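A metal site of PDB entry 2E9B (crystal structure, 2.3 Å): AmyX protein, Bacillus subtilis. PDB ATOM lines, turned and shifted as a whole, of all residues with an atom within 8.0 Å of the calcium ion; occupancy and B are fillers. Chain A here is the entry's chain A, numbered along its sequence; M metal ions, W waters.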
ATOM      1  N   VAL A 185     -34.695 -17.790  16.415  1.00  0.00           N
ATOM      2  CA  VAL A 185     -34.042 -16.501  16.668  1.00  0.00           C
ATOM      3  C   VAL A 185     -32.922 -16.221  15.691  1.00  0.00           C
ATOM      4  O   VAL A 185     -32.461 -17.132  14.996  1.00  0.00           O
ATOM      5  CB  VAL A 185     -33.439 -16.461  18.097  1.00  0.00           C
ATOM      6  CG1 VAL A 185     -34.565 -16.575  19.145  1.00  0.00           C
ATOM      7  CG2 VAL A 185     -32.419 -17.581  18.270  1.00  0.00           C
ATOM      8  N   THR A 186     -32.485 -14.967  15.622  1.00  0.00           N
ATOM      9  CA  THR A 186     -31.409 -14.566  14.724  1.00  0.00           C
ATOM     10  C   THR A 186     -30.040 -14.898  15.355  1.00  0.00           C
ATOM     11  O   THR A 186     -29.974 -15.294  16.509  1.00  0.00           O
ATOM     12  CB  THR A 186     -31.494 -13.061  14.408  1.00  0.00           C
ATOM     13  OG1 THR A 186     -31.503 -12.302  15.629  1.00  0.00           O
ATOM     14  CG2 THR A 186     -32.761 -12.752  13.628  1.00  0.00           C
ATOM     15  N   VAL A 187     -28.952 -14.722  14.605  1.00  0.00           N
ATOM     16  CA  VAL A 187     -27.623 -15.005  15.133  1.00  0.00           C
ATOM     17  C   VAL A 187     -27.381 -14.284  16.461  1.00  0.00           C
ATOM     18  O   VAL A 187     -27.652 -13.088  16.591  1.00  0.00           O
ATOM     19  CB  VAL A 187     -26.518 -14.629  14.095  1.00  0.00           C
ATOM     20  CG1 VAL A 187     -26.574 -13.160  13.758  1.00  0.00           C
ATOM     21  CG2 VAL A 187     -25.142 -14.996  14.645  1.00  0.00           C
ATOM     22  N   ASN A 188     -26.883 -15.032  17.446  1.00  0.00           N
ATOM     23  CA  ASN A 188     -26.622 -14.525  18.792  1.00  0.00           C
ATOM     24  C   ASN A 188     -27.906 -14.174  19.556  1.00  0.00           C
ATOM     25  O   ASN A 188     -27.871 -13.535  20.609  1.00  0.00           O
ATOM     26  CB  ASN A 188     -25.667 -13.330  18.774  1.00  0.00           C
ATOM     27  CG  ASN A 188     -24.214 -13.743  18.632  1.00  0.00           C
ATOM     28  OD1 ASN A 188     -23.778 -14.727  19.233  1.00  0.00           O
ATOM     29  ND2 ASN A 188     -23.446 -12.982  17.856  1.00  0.00           N
ATOM     30  N   GLY A 189     -29.047 -14.595  18.998  1.00  0.00           N
ATOM     31  CA  GLY A 189     -30.339 -14.369  19.632  1.00  0.00           C
ATOM     32  C   GLY A 189     -30.764 -12.936  19.893  1.00  0.00           C
ATOM     33  O   GLY A 189     -31.355 -12.648  20.939  1.00  0.00           O
ATOM     34  N   ASN A 274     -30.552 -25.299  24.560  1.00  0.00           N
ATOM     35  CA  ASN A 274     -31.432 -24.159  24.317  1.00  0.00           C
ATOM     36  C   ASN A 274     -30.427 -23.015  24.111  1.00  0.00           C
ATOM     37  O   ASN A 274     -29.272 -23.147  24.503  1.00  0.00           O
ATOM     38  CB  ASN A 274     -32.345 -23.896  25.531  1.00  0.00           C
ATOM     39  CG  ASN A 274     -31.569 -23.449  26.774  1.00  0.00           C
ATOM     40  OD1 ASN A 274     -31.493 -22.262  27.081  1.00  0.00           O
ATOM     41  ND2 ASN A 274     -31.001 -24.415  27.484  1.00  0.00           N
ATOM     42  N   ASP A 275     -30.847 -21.913  23.492  1.00  0.00           N
ATOM     43  CA  ASP A 275     -29.888 -20.833  23.255  1.00  0.00           C
ATOM     44  C   ASP A 275     -29.338 -20.211  24.531  1.00  0.00           C
ATOM     45  O   ASP A 275     -30.096 -19.788  25.411  1.00  0.00           O
ATOM     46  CB  ASP A 275     -30.497 -19.718  22.390  1.00  0.00           C
ATOM     47  CG  ASP A 275     -29.428 -18.779  21.827  1.00  0.00           C
ATOM     48  OD1 ASP A 275     -29.731 -17.623  21.489  1.00  0.00           O
ATOM     49  OD2 ASP A 275     -28.268 -19.217  21.700  1.00  0.00           O
ATOM     50  N   PHE A 276     -28.011 -20.152  24.616  1.00  0.00           N
ATOM     51  CA  PHE A 276     -27.335 -19.575  25.759  1.00  0.00           C
ATOM     52  C   PHE A 276     -26.297 -18.525  25.344  1.00  0.00           C
ATOM     53  O   PHE A 276     -26.025 -18.338  24.155  1.00  0.00           O
ATOM     54  CB  PHE A 276     -26.642 -20.667  26.606  1.00  0.00           C
ATOM     55  CG  PHE A 276     -25.699 -21.545  25.818  1.00  0.00           C
ATOM     56  CD1 PHE A 276     -26.125 -22.775  25.328  1.00  0.00           C
ATOM     57  CD2 PHE A 276     -24.382 -21.142  25.586  1.00  0.00           C
ATOM     58  CE1 PHE A 276     -25.255 -23.607  24.611  1.00  0.00           C
ATOM     59  CE2 PHE A 276     -23.497 -21.970  24.876  1.00  0.00           C
ATOM     60  CZ  PHE A 276     -23.938 -23.204  24.379  1.00  0.00           C
ATOM     61  N   ALA A 277     -25.724 -17.859  26.341  1.00  0.00           N
ATOM     62  CA  ALA A 277     -24.707 -16.843  26.119  1.00  0.00           C
ATOM     63  C   ALA A 277     -23.343 -17.364  26.574  1.00  0.00           C
ATOM     64  O   ALA A 277     -23.273 -18.251  27.421  1.00  0.00           O
ATOM     65  CB  ALA A 277     -25.069 -15.585  26.895  1.00  0.00           C
ATOM     66  N   GLY A 278     -22.270 -16.805  26.019  1.00  0.00           N
ATOM     67  CA  GLY A 278     -20.939 -17.244  26.403  1.00  0.00           C
ATOM     68  C   GLY A 278     -20.035 -17.556  25.218  1.00  0.00           C
ATOM     69  O   GLY A 278     -18.819 -17.593  25.348  1.00  0.00           O
ATOM     70  N   VAL A 279     -20.651 -17.815  24.069  1.00  0.00           N
ATOM     71  CA  VAL A 279     -19.895 -18.109  22.859  1.00  0.00           C
ATOM     72  C   VAL A 279     -20.462 -17.270  21.729  1.00  0.00           C
ATOM     73  O   VAL A 279     -21.670 -17.228  21.532  1.00  0.00           O
ATOM     74  CB  VAL A 279     -19.999 -19.606  22.496  1.00  0.00           C
ATOM     75  CG1 VAL A 279     -19.321 -19.875  21.153  1.00  0.00           C
ATOM     76  CG2 VAL A 279     -19.355 -20.455  23.577  1.00  0.00           C
ATOM     77  N   ASP A 280     -19.587 -16.594  20.990  1.00  0.00           N
ATOM     78  CA  ASP A 280     -20.007 -15.777  19.861  1.00  0.00           C
ATOM     79  C   ASP A 280     -20.291 -16.750  18.722  1.00  0.00           C
ATOM     80  O   ASP A 280     -19.378 -17.432  18.244  1.00  0.00           O
ATOM     81  CB  ASP A 280     -18.895 -14.805  19.451  1.00  0.00           C
ATOM     82  CG  ASP A 280     -19.306 -13.898  18.296  1.00  0.00           C
ATOM     83  OD1 ASP A 280     -20.250 -14.257  17.567  1.00  0.00           O
ATOM     84  OD2 ASP A 280     -18.668 -12.834  18.110  1.00  0.00           O
ATOM     85  N   GLU A 281     -21.546 -16.813  18.282  1.00  0.00           N
ATOM     86  CA  GLU A 281     -21.922 -17.737  17.222  1.00  0.00           C
ATOM     87  C   GLU A 281     -21.293 -17.367  15.877  1.00  0.00           C
ATOM     88  O   GLU A 281     -21.235 -18.187  14.962  1.00  0.00           O
ATOM     89  CB  GLU A 281     -23.459 -17.808  17.131  1.00  0.00           C
ATOM     90  CG  GLU A 281     -24.117 -17.859  18.521  1.00  0.00           C
ATOM     91  CD  GLU A 281     -25.613 -18.187  18.503  1.00  0.00           C
ATOM     92  OE1 GLU A 281     -26.325 -17.785  17.562  1.00  0.00           O
ATOM     93  OE2 GLU A 281     -26.081 -18.855  19.451  1.00  0.00           O
ATOM     94  N   ASN A 293     -26.277 -20.511  30.823  1.00  0.00           N
ATOM     95  CA  ASN A 293     -26.615 -19.079  30.825  1.00  0.00           C
ATOM     96  C   ASN A 293     -27.783 -18.889  29.850  1.00  0.00           C
ATOM     97  O   ASN A 293     -27.587 -18.355  28.741  1.00  0.00           O
ATOM     98  CB  ASN A 293     -25.417 -18.237  30.364  1.00  0.00           C
ATOM     99  CG  ASN A 293     -24.159 -18.544  31.148  1.00  0.00           C
ATOM    100  OD1 ASN A 293     -24.133 -18.454  32.376  1.00  0.00           O
ATOM    101  ND2 ASN A 293     -23.100 -18.918  30.435  1.00  0.00           N
ATOM    102  N   LEU A 295     -30.869 -17.813  27.572  1.00  0.00           N
ATOM    103  CA  LEU A 295     -31.319 -16.624  26.860  1.00  0.00           C
ATOM    104  C   LEU A 295     -32.723 -16.888  26.329  1.00  0.00           C
ATOM    105  O   LEU A 295     -33.658 -16.126  26.566  1.00  0.00           O
ATOM    106  CB  LEU A 295     -30.398 -16.296  25.675  1.00  0.00           C
ATOM    107  CG  LEU A 295     -29.036 -15.661  25.986  1.00  0.00           C
ATOM    108  CD1 LEU A 295     -28.305 -15.329  24.673  1.00  0.00           C
ATOM    109  CD2 LEU A 295     -29.240 -14.396  26.804  1.00  0.00           C
ATOM    110  N   HIS A 296     -32.870 -17.997  25.597  1.00  0.00           N
ATOM    111  CA  HIS A 296     -34.160 -18.370  25.025  1.00  0.00           C
ATOM    112  C   HIS A 296     -34.457 -19.846  25.292  1.00  0.00           C
ATOM    113  O   HIS A 296     -33.773 -20.728  24.770  1.00  0.00           O
ATOM    114  CB  HIS A 296     -34.139 -18.092  23.526  1.00  0.00           C
ATOM    115  CG  HIS A 296     -33.691 -16.707  23.191  1.00  0.00           C
ATOM    116  ND1 HIS A 296     -34.379 -15.580  23.602  1.00  0.00           N
ATOM    117  CD2 HIS A 296     -32.590 -16.258  22.534  1.00  0.00           C
ATOM    118  CE1 HIS A 296     -33.717 -14.502  23.214  1.00  0.00           C
ATOM    119  NE2 HIS A 296     -32.633 -14.879  22.569  1.00  0.00           N
ATOM    120  N   PRO A 300     -33.103 -23.380  19.928  1.00  0.00           N
ATOM    121  CA  PRO A 300     -31.793 -24.042  19.997  1.00  0.00           C
ATOM    122  C   PRO A 300     -30.597 -23.085  19.964  1.00  0.00           C
ATOM    123  O   PRO A 300     -30.704 -21.974  19.450  1.00  0.00           O
ATOM    124  CB  PRO A 300     -31.786 -24.958  18.766  1.00  0.00           C
ATOM    125  CG  PRO A 300     -33.241 -24.988  18.299  1.00  0.00           C
ATOM    126  CD  PRO A 300     -33.723 -23.603  18.605  1.00  0.00           C
ATOM    127  N   GLU A 301     -29.457 -23.547  20.487  1.00  0.00           N
ATOM    128  CA  GLU A 301     -28.209 -22.783  20.514  1.00  0.00           C
ATOM    129  C   GLU A 301     -27.639 -22.689  19.100  1.00  0.00           C
ATOM    130  O   GLU A 301     -27.691 -23.659  18.344  1.00  0.00           O
ATOM    131  CB  GLU A 301     -27.180 -23.467  21.434  1.00  0.00           C
ATOM    132  CG  GLU A 301     -25.716 -23.088  21.171  1.00  0.00           C
ATOM    133  CD  GLU A 301     -25.384 -21.634  21.525  1.00  0.00           C
ATOM    134  OE1 GLU A 301     -24.304 -21.170  21.123  1.00  0.00           O
ATOM    135  OE2 GLU A 301     -26.195 -20.969  22.198  1.00  0.00           O
ATOM    136  N   GLY A 302     -27.067 -21.542  18.753  1.00  0.00           N
ATOM    137  CA  GLY A 302     -26.531 -21.371  17.411  1.00  0.00           C
ATOM    138  C   GLY A 302     -25.131 -21.847  17.075  1.00  0.00           C
ATOM    139  O   GLY A 302     -24.864 -22.218  15.934  1.00  0.00           O
ATOM    140  N   SER A 303     -24.223 -21.863  18.048  1.00  0.00           N
ATOM    141  CA  SER A 303     -22.847 -22.281  17.762  1.00  0.00           C
ATOM    142  C   SER A 303     -22.677 -23.754  17.367  1.00  0.00           C
ATOM    143  O   SER A 303     -21.621 -24.122  16.845  1.00  0.00           O
ATOM    144  CB  SER A 303     -21.938 -21.972  18.971  1.00  0.00           C
ATOM    145  OG  SER A 303     -22.151 -22.914  20.019  1.00  0.00           O
ATOM    146  N   TYR A 304     -23.684 -24.584  17.607  1.00  0.00           N
ATOM    147  CA  TYR A 304     -23.573 -25.996  17.252  1.00  0.00           C
ATOM    148  C   TYR A 304     -24.108 -26.300  15.852  1.00  0.00           C
ATOM    149  O   TYR A 304     -24.021 -27.438  15.380  1.00  0.00           O
ATOM    150  CB  TYR A 304     -24.302 -26.878  18.282  1.00  0.00           C
ATOM    151  CG  TYR A 304     -23.828 -26.750  19.727  1.00  0.00           C
ATOM    152  CD1 TYR A 304     -22.460 -26.698  20.040  1.00  0.00           C
ATOM    153  CD2 TYR A 304     -24.740 -26.724  20.780  1.00  0.00           C
ATOM    154  CE1 TYR A 304     -22.022 -26.621  21.389  1.00  0.00           C
ATOM    155  CE2 TYR A 304     -24.325 -26.637  22.118  1.00  0.00           C
ATOM    156  CZ  TYR A 304     -22.966 -26.588  22.411  1.00  0.00           C
ATOM    157  OH  TYR A 304     -22.575 -26.491  23.738  1.00  0.00           O
ATOM    158  N   ARG A 314     -30.443 -24.471  12.381  1.00  0.00           N
ATOM    159  CA  ARG A 314     -30.160 -25.074  13.672  1.00  0.00           C
ATOM    160  C   ARG A 314     -31.256 -26.036  14.147  1.00  0.00           C
ATOM    161  O   ARG A 314     -30.976 -27.027  14.826  1.00  0.00           O
ATOM    162  CB  ARG A 314     -29.918 -23.992  14.729  1.00  0.00           C
ATOM    163  CG  ARG A 314     -31.142 -23.167  15.089  1.00  0.00           C
ATOM    164  CD  ARG A 314     -30.777 -22.087  16.097  1.00  0.00           C
ATOM    165  NE  ARG A 314     -29.991 -20.994  15.510  1.00  0.00           N
ATOM    166  CZ  ARG A 314     -29.497 -19.976  16.202  1.00  0.00           C
ATOM    167  NH1 ARG A 314     -29.703 -19.892  17.510  1.00  0.00           N
ATOM    168  NH2 ARG A 314     -28.810 -19.021  15.597  1.00  0.00           N
HETATM  169 CA    CA M   1     -25.985 -18.609  21.816  1.00  0.00          CA
HETATM  170  O   HOH W   1     -23.749 -18.858  22.053  1.00  0.00           O
HETATM  171  O   HOH W   2     -27.097 -16.536  21.797  1.00  0.00           O
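N of Leu 295 is in hydrogen-bond range of O of Asp 275, at 3.0 Å.
The backbone carbonyl oxygen (O) of Asp 275 sits at hydrogen-bond distance from the backbone NH (N) of His 296.
The side-chain carboxylate (OE2) of Glu 281 sits close to the backbone NH (N) of Gly 302, at 2.9 Å.
The backbone NH of Asn 188 lies within hydrogen-bond range of the side-chain carboxylate of Glu 281 (2.8 Å).
NH2 of Arg 314 is in salt-bridge range of OE1 of Glu 281.
The side-chain hydroxyl (OG) of Ser 303 sits at hydrogen-bond distance from the side-chain carboxylate (OE1) of Glu 301 (3.0 Å).
The calcium ion is bound by water W1, water W2, O of Phe 276, OD2 of Asp 275, OE2 of Glu 281 and OE2 of Glu 301.
The calcium ion has six donor atoms within binding distance.
Slightly farther from the calcium ion lies the side-chain carboxylate (OE1) of Glu 301 (3.1 Å).
Of the 22 residues printed, 4 come within 4 Å of the calcium ion.
Water W1 lies within hydrogen-bond range of OE1 of Glu 301 (2.6 Å) and O of Val 279 (2.7 Å).
Water W2 lies within hydrogen-bond range of OD1 of Asp 275 (2.9 Å) and O of Asn 188 (3.3 Å).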
